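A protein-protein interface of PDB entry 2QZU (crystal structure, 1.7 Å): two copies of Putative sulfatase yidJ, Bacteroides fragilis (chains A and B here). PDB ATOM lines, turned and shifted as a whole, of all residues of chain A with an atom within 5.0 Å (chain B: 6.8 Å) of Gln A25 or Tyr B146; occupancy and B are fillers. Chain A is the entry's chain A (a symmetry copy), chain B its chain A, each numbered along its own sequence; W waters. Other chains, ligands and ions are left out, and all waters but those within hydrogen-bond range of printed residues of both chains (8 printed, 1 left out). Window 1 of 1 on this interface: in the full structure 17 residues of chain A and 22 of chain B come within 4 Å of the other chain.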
ATOM      1  N   GLU A  23      20.816  18.153   6.288  1.00  0.00           N
ATOM      2  CA  GLU A  23      20.245  19.336   6.897  1.00  0.00           C
ATOM      3  C   GLU A  23      20.202  20.572   6.015  1.00  0.00           C
ATOM      4  O   GLU A  23      21.183  20.942   5.371  1.00  0.00           O
ATOM      5  CB  GLU A  23      21.005  19.631   8.184  1.00  0.00           C
ATOM      6  CG  GLU A  23      20.992  18.445   9.123  1.00  0.00           C
ATOM      7  CD  GLU A  23      21.851  18.652  10.344  1.00  0.00           C
ATOM      8  OE1 GLU A  23      23.093  18.677  10.203  1.00  0.00           O
ATOM      9  OE2 GLU A  23      21.282  18.794  11.444  1.00  0.00           O
ATOM     10  N   LYS A  24      19.036  21.202   6.000  1.00  0.00           N
ATOM     11  CA  LYS A  24      18.809  22.411   5.231  1.00  0.00           C
ATOM     12  C   LYS A  24      19.513  23.560   5.944  1.00  0.00           C
ATOM     13  O   LYS A  24      19.531  23.613   7.176  1.00  0.00           O
ATOM     14  CB  LYS A  24      17.306  22.671   5.152  1.00  0.00           C
ATOM     15  CG  LYS A  24      16.899  23.923   4.411  1.00  0.00           C
ATOM     16  CD  LYS A  24      15.384  24.012   4.371  1.00  0.00           C
ATOM     17  CE  LYS A  24      14.909  25.308   3.754  1.00  0.00           C
ATOM     18  NZ  LYS A  24      13.423  25.369   3.724  1.00  0.00           N
ATOM     19  N   GLN A  25      20.111  24.470   5.182  1.00  0.00           N
ATOM     20  CA  GLN A  25      20.790  25.607   5.790  1.00  0.00           C
ATOM     21  C   GLN A  25      19.733  26.485   6.458  1.00  0.00           C
ATOM     22  O   GLN A  25      18.623  26.625   5.942  1.00  0.00           O
ATOM     23  CB  GLN A  25      21.552  26.411   4.731  1.00  0.00           C
ATOM     24  CG  GLN A  25      22.780  25.705   4.172  1.00  0.00           C
ATOM     25  CD  GLN A  25      23.821  25.406   5.240  1.00  0.00           C
ATOM     26  OE1 GLN A  25      23.611  24.562   6.112  1.00  0.00           O
ATOM     27  NE2 GLN A  25      24.949  26.104   5.177  1.00  0.00           N
ATOM     28  N   PRO A  26      20.059  27.083   7.615  1.00  0.00           N
ATOM     29  CA  PRO A  26      19.106  27.942   8.333  1.00  0.00           C
ATOM     30  C   PRO A  26      18.800  29.297   7.677  1.00  0.00           C
ATOM     31  O   PRO A  26      17.876  29.999   8.098  1.00  0.00           O
ATOM     32  CB  PRO A  26      19.746  28.079   9.714  1.00  0.00           C
ATOM     33  CG  PRO A  26      21.201  28.024   9.408  1.00  0.00           C
ATOM     34  CD  PRO A  26      21.296  26.906   8.397  1.00  0.00           C
ATOM     35  N   THR A  27      19.580  29.659   6.662  1.00  0.00           N
ATOM     36  CA  THR A  27      19.367  30.903   5.921  1.00  0.00           C
ATOM     37  C   THR A  27      19.430  30.544   4.436  1.00  0.00           C
ATOM     38  O   THR A  27      20.205  29.682   4.032  1.00  0.00           O
ATOM     39  CB  THR A  27      20.423  31.979   6.273  1.00  0.00           C
ATOM     40  OG1 THR A  27      21.736  31.495   5.977  1.00  0.00           O
ATOM     41  CG2 THR A  27      20.339  32.332   7.750  1.00  0.00           C
ATOM     42  N   GLN A 218      25.702  21.842  -0.963  1.00  0.00           N
ATOM     43  CA  GLN A 218      25.069  22.639   0.088  1.00  0.00           C
ATOM     44  C   GLN A 218      25.821  22.651   1.419  1.00  0.00           C
ATOM     45  O   GLN A 218      25.199  22.623   2.477  1.00  0.00           O
ATOM     46  CB  GLN A 218      23.640  22.142   0.345  1.00  0.00           C
ATOM     47  CG  GLN A 218      22.720  22.156  -0.865  1.00  0.00           C
ATOM     48  CD  GLN A 218      21.304  21.717  -0.520  1.00  0.00           C
ATOM     49  OE1 GLN A 218      20.593  22.397   0.223  1.00  0.00           O
ATOM     50  NE2 GLN A 218      20.895  20.570  -1.050  1.00  0.00           N
ATOM     51  N   LYS A 219      27.147  22.701   1.378  1.00  0.00           N
ATOM     52  CA  LYS A 219      27.916  22.722   2.619  1.00  0.00           C
ATOM     53  C   LYS A 219      27.858  24.099   3.276  1.00  0.00           C
ATOM     54  O   LYS A 219      28.107  24.239   4.474  1.00  0.00           O
ATOM     55  CB  LYS A 219      29.373  22.329   2.357  1.00  0.00           C
ATOM     56  CG  LYS A 219      30.123  23.278   1.446  1.00  0.00           C
ATOM     57  CD  LYS A 219      31.577  22.860   1.305  1.00  0.00           C
ATOM     58  CE  LYS A 219      32.316  23.787   0.357  1.00  0.00           C
ATOM     59  NZ  LYS A 219      33.753  23.422   0.223  1.00  0.00           N
ATOM     60  N   GLN A 220      27.524  25.111   2.482  1.00  0.00           N
ATOM     61  CA  GLN A 220      27.420  26.481   2.973  1.00  0.00           C
ATOM     62  C   GLN A 220      26.464  27.253   2.073  1.00  0.00           C
ATOM     63  O   GLN A 220      26.190  26.832   0.952  1.00  0.00           O
ATOM     64  CB  GLN A 220      28.794  27.158   2.949  1.00  0.00           C
ATOM     65  CG  GLN A 220      29.450  27.173   1.575  1.00  0.00           C
ATOM     66  CD  GLN A 220      30.820  27.823   1.587  1.00  0.00           C
ATOM     67  OE1 GLN A 220      30.948  29.026   1.815  1.00  0.00           O
ATOM     68  NE2 GLN A 220      31.854  27.030   1.342  1.00  0.00           N
ATOM     69  N   PRO A 221      25.921  28.381   2.559  1.00  0.00           N
ATOM     70  CA  PRO A 221      25.010  29.134   1.692  1.00  0.00           C
ATOM     71  C   PRO A 221      25.834  29.899   0.657  1.00  0.00           C
ATOM     72  O   PRO A 221      27.054  30.025   0.795  1.00  0.00           O
ATOM     73  CB  PRO A 221      24.309  30.090   2.658  1.00  0.00           C
ATOM     74  CG  PRO A 221      24.470  29.433   4.010  1.00  0.00           C
ATOM     75  CD  PRO A 221      25.867  28.885   3.941  1.00  0.00           C
ATOM     76  N   ASN A 305      15.003  26.735  -1.919  1.00  0.00           N
ATOM     77  CA  ASN A 305      15.464  27.512  -0.774  1.00  0.00           C
ATOM     78  C   ASN A 305      16.474  28.566  -1.162  1.00  0.00           C
ATOM     79  O   ASN A 305      17.480  28.777  -0.480  1.00  0.00           O
ATOM     80  CB  ASN A 305      16.053  26.623   0.322  1.00  0.00           C
ATOM     81  CG  ASN A 305      16.186  27.364   1.642  1.00  0.00           C
ATOM     82  OD1 ASN A 305      15.246  28.042   2.076  1.00  0.00           O
ATOM     83  ND2 ASN A 305      17.343  27.244   2.284  1.00  0.00           N
ATOM     84  N   GLN A 345       9.359  29.738   1.167  1.00  0.00           N
ATOM     85  CA  GLN A 345       8.714  30.690   2.066  1.00  0.00           C
ATOM     86  C   GLN A 345       7.650  31.602   1.478  1.00  0.00           C
ATOM     87  O   GLN A 345       6.882  32.211   2.222  1.00  0.00           O
ATOM     88  CB  GLN A 345       9.777  31.562   2.735  1.00  0.00           C
ATOM     89  CG  GLN A 345      10.591  30.842   3.787  1.00  0.00           C
ATOM     90  CD  GLN A 345       9.728  30.337   4.922  1.00  0.00           C
ATOM     91  OE1 GLN A 345       8.915  31.080   5.471  1.00  0.00           O
ATOM     92  NE2 GLN A 345       9.902  29.073   5.283  1.00  0.00           N
ATOM     93  N   VAL B 143       4.736  20.273  10.511  1.00  0.00           N
ATOM     94  CA  VAL B 143       4.598  21.484  11.310  1.00  0.00           C
ATOM     95  C   VAL B 143       5.269  22.618  10.543  1.00  0.00           C
ATOM     96  O   VAL B 143       6.235  22.400   9.804  1.00  0.00           O
ATOM     97  CB  VAL B 143       5.230  21.338  12.716  1.00  0.00           C
ATOM     98  CG1 VAL B 143       4.477  20.279  13.514  1.00  0.00           C
ATOM     99  CG2 VAL B 143       6.697  20.984  12.609  1.00  0.00           C
ATOM    100  N   ASP B 144       4.758  23.827  10.735  1.00  0.00           N
ATOM    101  CA  ASP B 144       5.234  25.003  10.013  1.00  0.00           C
ATOM    102  C   ASP B 144       6.547  25.692  10.399  1.00  0.00           C
ATOM    103  O   ASP B 144       6.541  26.845  10.835  1.00  0.00           O
ATOM    104  CB  ASP B 144       4.099  26.038   9.980  1.00  0.00           C
ATOM    105  CG  ASP B 144       4.366  27.175   9.012  1.00  0.00           C
ATOM    106  OD1 ASP B 144       4.892  26.908   7.912  1.00  0.00           O
ATOM    107  OD2 ASP B 144       4.036  28.334   9.348  1.00  0.00           O
ATOM    108  N   THR B 145       7.670  24.993  10.238  1.00  0.00           N
ATOM    109  CA  THR B 145       8.983  25.594  10.497  1.00  0.00           C
ATOM    110  C   THR B 145       9.752  25.538   9.178  1.00  0.00           C
ATOM    111  O   THR B 145       9.446  24.713   8.315  1.00  0.00           O
ATOM    112  CB  THR B 145       9.779  24.868  11.612  1.00  0.00           C
ATOM    113  OG1 THR B 145       9.846  23.469  11.335  1.00  0.00           O
ATOM    114  CG2 THR B 145       9.122  25.106  12.966  1.00  0.00           C
ATOM    115  N   TYR B 146      10.743  26.411   9.020  1.00  0.00           N
ATOM    116  CA  TYR B 146      11.498  26.492   7.769  1.00  0.00           C
ATOM    117  C   TYR B 146      12.093  25.190   7.237  1.00  0.00           C
ATOM    118  O   TYR B 146      12.114  24.972   6.022  1.00  0.00           O
ATOM    119  CB  TYR B 146      12.615  27.540   7.881  1.00  0.00           C
ATOM    120  CG  TYR B 146      13.867  27.016   8.535  1.00  0.00           C
ATOM    121  CD1 TYR B 146      13.974  26.955   9.923  1.00  0.00           C
ATOM    122  CD2 TYR B 146      14.912  26.501   7.766  1.00  0.00           C
ATOM    123  CE1 TYR B 146      15.083  26.386  10.529  1.00  0.00           C
ATOM    124  CE2 TYR B 146      16.020  25.928   8.359  1.00  0.00           C
ATOM    125  CZ  TYR B 146      16.097  25.870   9.747  1.00  0.00           C
ATOM    126  OH  TYR B 146      17.153  25.252  10.360  1.00  0.00           O
ATOM    127  N   ASN B 147      12.583  24.330   8.128  1.00  0.00           N
ATOM    128  CA  ASN B 147      13.195  23.077   7.699  1.00  0.00           C
ATOM    129  C   ASN B 147      12.207  21.972   7.341  1.00  0.00           C
ATOM    130  O   ASN B 147      12.585  20.809   7.207  1.00  0.00           O
ATOM    131  CB  ASN B 147      14.202  22.586   8.749  1.00  0.00           C
ATOM    132  CG  ASN B 147      13.611  22.472  10.151  1.00  0.00           C
ATOM    133  OD1 ASN B 147      12.553  23.025  10.453  1.00  0.00           O
ATOM    134  ND2 ASN B 147      14.318  21.761  11.024  1.00  0.00           N
ATOM    135  N   ASN B 148      10.942  22.347   7.181  1.00  0.00           N
ATOM    136  CA  ASN B 148       9.905  21.396   6.803  1.00  0.00           C
ATOM    137  C   ASN B 148       9.301  21.792   5.463  1.00  0.00           C
ATOM    138  O   ASN B 148       8.349  21.173   4.986  1.00  0.00           O
ATOM    139  CB  ASN B 148       8.818  21.326   7.872  1.00  0.00           C
ATOM    140  CG  ASN B 148       9.210  20.442   9.036  1.00  0.00           C
ATOM    141  OD1 ASN B 148      10.324  19.908   9.081  1.00  0.00           O
ATOM    142  ND2 ASN B 148       8.298  20.276   9.983  1.00  0.00           N
ATOM    143  N   ARG B 149       9.863  22.838   4.864  1.00  0.00           N
ATOM    144  CA  ARG B 149       9.420  23.315   3.559  1.00  0.00           C
ATOM    145  C   ARG B 149      10.299  22.640   2.512  1.00  0.00           C
ATOM    146  O   ARG B 149      11.503  22.473   2.715  1.00  0.00           O
ATOM    147  CB  ARG B 149       9.587  24.835   3.446  1.00  0.00           C
ATOM    148  CG  ARG B 149       8.726  25.662   4.390  1.00  0.00           C
ATOM    149  CD  ARG B 149       7.237  25.448   4.137  1.00  0.00           C
ATOM    150  NE  ARG B 149       6.410  26.292   4.998  1.00  0.00           N
ATOM    151  CZ  ARG B 149       5.985  27.511   4.676  1.00  0.00           C
ATOM    152  NH1 ARG B 149       6.302  28.040   3.501  1.00  0.00           N
ATOM    153  NH2 ARG B 149       5.240  28.204   5.529  1.00  0.00           N
ATOM    154  N   GLY B 150       9.702  22.252   1.393  1.00  0.00           N
ATOM    155  CA  GLY B 150      10.477  21.611   0.350  1.00  0.00           C
ATOM    156  C   GLY B 150      10.250  20.116   0.244  1.00  0.00           C
ATOM    157  O   GLY B 150       9.251  19.588   0.730  1.00  0.00           O
ATOM    158  N   VAL B 152      12.098  17.569   1.596  1.00  0.00           N
ATOM    159  CA  VAL B 152      12.316  16.808   2.825  1.00  0.00           C
ATOM    160  C   VAL B 152      12.109  17.613   4.110  1.00  0.00           C
ATOM    161  O   VAL B 152      12.699  18.683   4.284  1.00  0.00           O
ATOM    162  CB  VAL B 152      13.747  16.211   2.841  1.00  0.00           C
ATOM    163  CG1 VAL B 152      13.967  15.409   4.112  1.00  0.00           C
ATOM    164  CG2 VAL B 152      13.959  15.333   1.605  1.00  0.00           C
ATOM    165  N   THR B 174      14.230  19.298  15.472  1.00  0.00           N
ATOM    166  CA  THR B 174      15.499  19.876  15.047  1.00  0.00           C
ATOM    167  C   THR B 174      15.155  21.192  14.360  1.00  0.00           C
ATOM    168  O   THR B 174      14.090  21.326  13.757  1.00  0.00           O
ATOM    169  CB  THR B 174      16.331  18.932  14.132  1.00  0.00           C
ATOM    170  OG1 THR B 174      17.679  19.425  14.062  1.00  0.00           O
ATOM    171  CG2 THR B 174      15.743  18.843  12.735  1.00  0.00           C
ATOM    172  N   TYR B 175      16.043  22.173  14.489  1.00  0.00           N
ATOM    173  CA  TYR B 175      15.830  23.519  13.947  1.00  0.00           C
ATOM    174  C   TYR B 175      17.159  24.223  14.191  1.00  0.00           C
ATOM    175  O   TYR B 175      17.644  24.243  15.328  1.00  0.00           O
ATOM    176  CB  TYR B 175      14.714  24.192  14.744  1.00  0.00           C
ATOM    177  CG  TYR B 175      14.403  25.621  14.372  1.00  0.00           C
ATOM    178  CD1 TYR B 175      13.410  25.924  13.438  1.00  0.00           C
ATOM    179  CD2 TYR B 175      15.061  26.675  15.001  1.00  0.00           C
ATOM    180  CE1 TYR B 175      13.076  27.252  13.152  1.00  0.00           C
ATOM    181  CE2 TYR B 175      14.740  27.991  14.721  1.00  0.00           C
ATOM    182  CZ  TYR B 175      13.749  28.276  13.804  1.00  0.00           C
ATOM    183  OH  TYR B 175      13.413  29.589  13.573  1.00  0.00           O
ATOM    184  N   ASP B 176      17.722  24.840  13.153  1.00  0.00           N
ATOM    185  CA  ASP B 176      19.046  25.433  13.285  1.00  0.00           C
ATOM    186  C   ASP B 176      19.260  26.935  13.191  1.00  0.00           C
ATOM    187  O   ASP B 176      20.404  27.380  13.087  1.00  0.00           O
ATOM    188  CB  ASP B 176      19.994  24.729  12.307  1.00  0.00           C
ATOM    189  CG  ASP B 176      19.878  23.213  12.377  1.00  0.00           C
ATOM    190  OD1 ASP B 176      19.652  22.690  13.486  1.00  0.00           O
ATOM    191  OD2 ASP B 176      20.014  22.540  11.334  1.00  0.00           O
ATOM    192  N   TYR B 177      18.185  27.719  13.223  1.00  0.00           N
ATOM    193  CA  TYR B 177      18.335  29.171  13.193  1.00  0.00           C
ATOM    194  C   TYR B 177      18.404  29.563  14.674  1.00  0.00           C
ATOM    195  O   TYR B 177      17.401  29.926  15.285  1.00  0.00           O
ATOM    196  CB  TYR B 177      17.129  29.826  12.514  1.00  0.00           C
ATOM    197  CG  TYR B 177      17.291  31.318  12.353  1.00  0.00           C
ATOM    198  CD1 TYR B 177      18.170  31.844  11.403  1.00  0.00           C
ATOM    199  CD2 TYR B 177      16.618  32.201  13.193  1.00  0.00           C
ATOM    200  CE1 TYR B 177      18.378  33.217  11.300  1.00  0.00           C
ATOM    201  CE2 TYR B 177      16.815  33.575  13.100  1.00  0.00           C
ATOM    202  CZ  TYR B 177      17.699  34.076  12.154  1.00  0.00           C
ATOM    203  OH  TYR B 177      17.911  35.433  12.081  1.00  0.00           O
ATOM    204  N   MET B 182      12.699  27.755  18.216  1.00  0.00           N
ATOM    205  CA  MET B 182      11.308  27.488  18.551  1.00  0.00           C
ATOM    206  C   MET B 182      11.246  26.291  19.484  1.00  0.00           C
ATOM    207  O   MET B 182      12.163  25.461  19.518  1.00  0.00           O
ATOM    208  CB  MET B 182      10.456  27.262  17.290  1.00  0.00           C
ATOM    209  CG  MET B 182      11.073  26.390  16.224  1.00  0.00           C
ATOM    210  SD  MET B 182      10.997  24.519  16.653  1.00  0.00           S
ATOM    211  CE  MET B 182      11.527  23.782  14.965  1.00  0.00           C
ATOM    212  N   TYR B 195       8.167  30.841  19.165  1.00  0.00           N
ATOM    213  CA  TYR B 195       9.515  31.299  18.866  1.00  0.00           C
ATOM    214  C   TYR B 195       9.997  32.193  20.004  1.00  0.00           C
ATOM    215  O   TYR B 195       9.193  32.837  20.682  1.00  0.00           O
ATOM    216  CB  TYR B 195       9.527  32.098  17.561  1.00  0.00           C
ATOM    217  CG  TYR B 195       9.355  31.267  16.312  1.00  0.00           C
ATOM    218  CD1 TYR B 195      10.420  30.536  15.782  1.00  0.00           C
ATOM    219  CD2 TYR B 195       8.122  31.210  15.658  1.00  0.00           C
ATOM    220  CE1 TYR B 195      10.262  29.770  14.632  1.00  0.00           C
ATOM    221  CE2 TYR B 195       7.954  30.446  14.507  1.00  0.00           C
ATOM    222  CZ  TYR B 195       9.025  29.730  14.002  1.00  0.00           C
ATOM    223  OH  TYR B 195       8.855  28.973  12.869  1.00  0.00           O
ATOM    224  N   THR B 233      25.742  23.669  12.889  1.00  0.00           N
ATOM    225  CA  THR B 233      25.608  24.713  11.884  1.00  0.00           C
ATOM    226  C   THR B 233      24.626  25.810  12.095  1.00  0.00           C
ATOM    227  O   THR B 233      23.572  25.658  12.724  1.00  0.00           O
ATOM    228  CB  THR B 233      25.382  24.176  10.476  1.00  0.00           C
ATOM    229  OG1 THR B 233      24.419  23.124  10.514  1.00  0.00           O
ATOM    230  CG2 THR B 233      26.706  23.708   9.878  1.00  0.00           C
ATOM    231  N   GLY B 234      24.992  26.902  11.441  1.00  0.00           N
ATOM    232  CA  GLY B 234      24.313  28.154  11.550  1.00  0.00           C
ATOM    233  C   GLY B 234      25.442  28.639  12.432  1.00  0.00           C
ATOM    234  O   GLY B 234      25.216  29.206  13.492  1.00  0.00           O
ATOM    235  N   GLU B 236      27.438  30.987  12.051  1.00  0.00           N
ATOM    236  CA  GLU B 236      27.455  32.440  12.176  1.00  0.00           C
ATOM    237  C   GLU B 236      26.342  32.969  13.068  1.00  0.00           C
ATOM    238  O   GLU B 236      26.347  34.140  13.457  1.00  0.00           O
ATOM    239  CB  GLU B 236      27.334  33.095  10.796  1.00  0.00           C
ATOM    240  CG  GLU B 236      25.897  33.231  10.278  1.00  0.00           C
ATOM    241  CD  GLU B 236      25.345  31.970   9.636  1.00  0.00           C
ATOM    242  OE1 GLU B 236      25.925  30.882   9.836  1.00  0.00           O
ATOM    243  OE2 GLU B 236      24.315  32.068   8.931  1.00  0.00           O
ATOM    244  N   TYR B 271      36.873  26.169   3.369  1.00  0.00           N
ATOM    245  CA  TYR B 271      35.699  25.931   4.196  1.00  0.00           C
ATOM    246  C   TYR B 271      36.114  25.885   5.668  1.00  0.00           C
ATOM    247  O   TYR B 271      35.451  26.467   6.530  1.00  0.00           O
ATOM    248  CB  TYR B 271      35.024  24.614   3.807  1.00  0.00           C
ATOM    249  CG  TYR B 271      33.733  24.354   4.562  1.00  0.00           C
ATOM    250  CD1 TYR B 271      32.612  25.168   4.372  1.00  0.00           C
ATOM    251  CD2 TYR B 271      33.641  23.315   5.489  1.00  0.00           C
ATOM    252  CE1 TYR B 271      31.435  24.953   5.088  1.00  0.00           C
ATOM    253  CE2 TYR B 271      32.471  23.092   6.210  1.00  0.00           C
ATOM    254  CZ  TYR B 271      31.372  23.913   6.007  1.00  0.00           C
ATOM    255  OH  TYR B 271      30.217  23.695   6.726  1.00  0.00           O
HETATM  256  O   HOH W   1      23.103  30.147   7.742  1.00  0.00           O
HETATM  257  O   HOH W   2      18.913  20.111  11.785  1.00  0.00           O
HETATM  258  O   HOH W   3       8.027  28.211   7.871  1.00  0.00           O
HETATM  259  O   HOH W   4      12.060  27.650   4.509  1.00  0.00           O
HETATM  260  O   HOH W   5      18.067  23.228   9.278  1.00  0.00           O
HETATM  261  O   HOH W   6      28.311  25.936   7.057  1.00  0.00           O
HETATM  262  O   HOH W   7       4.212  30.328   2.425  1.00  0.00           O
HETATM  263  O   HOH W   8      21.979  23.440   9.611  1.00  0.00           O
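NZ of Lys A24 is in hydrogen-bond range of O of Tyr B146 (2.7 Å).
O of Lys A219 lies within hydrogen-bond range of OH of Tyr B271, at 3.1 Å.
The guanidinium group (NH2) of Arg B149 is in salt-bridge range of the side-chain carboxylate (OD1) of Asp B144.
The side-chain hydroxyl (OH) of Tyr B146 is in hydrogen-bond range of the backbone NH (N) of Asp B176 (2.9 Å).
OD2 of Asp B176 touches OE2 of Glu A23, at 3.96 Å.
Arg B149 touches Lys A24 (O to NZ, 3.6 Å).
Tyr B146 touches Gln A25 (CE2 to O, 3.6 Å).
CA of Pro A26 touches CE2 of Tyr B146 (3.7 Å).
O of Asp B176 touches CB of Pro A26, 3.5 Å away.
Tyr B177 touches Pro A26 (CD1 to O, 3.8 Å).
Gly B234 touches Pro A26 (CA to CG, 3.8 Å).
Thr A27 touches Glu B236.
Tyr B146 touches Gln A345 (CA to NE2, 3.9 Å).
Arg B149 touches Gln A345.
Tyr B146 touches four residues of chain A.
Printed residues of chain A within 4 Å of Asp B176: Glu A23 and Pro A26.
Of the printed residues of chain B, Pro A26 touches Tyr B146 (3.7 Å), Asp B176 (3.5 Å), Tyr B177 (3.8 Å) and Gly B234 (3.8 Å).
The nearest residue of chain B that does not touch Gln A25 is Thr B233 (4.7 Å).
The nearest printed residue of chain A that does not touch Tyr B146 is Thr A27 (5.4 Å).
Hydrophobic or aromatic side chains of chain A that line the printed part of chain B: Pro A26.
Of the 19 printed residues of chain B, 7 touch a printed residue of chain A.
Printed residues of chain B that touch a printed residue of chain A: Tyr B146, Arg B149, Asp B176, Tyr B177, Gly B234, Glu B236 and Tyr B271.
No position is printed for both chains.
Water W1 bridges OE2 of Glu B236 (2.6 Å) and OG1 of Thr A27 (2.6 Å).
Water W8 lies within hydrogen-bond range of OG1 of Thr B233, OD2 of Asp B176 and O of Lys A24.
Water W2 lies within hydrogen-bond range of OG1 of Thr B174 (2.7 Å), OD2 of Asp B176 (2.7 Å) and OE2 of Glu A23 (2.7 Å).
Water W4 lies within hydrogen-bond range of the side-chain amide nitrogen of Gln A345, the side-chain amino group of Lys A24 and the backbone carbonyl oxygen of Tyr B146.
Water W6 bridges OH of Tyr B271 and O of Lys A219.
Water W7 bridges O of Gln A345 and NH1 of Arg B149.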
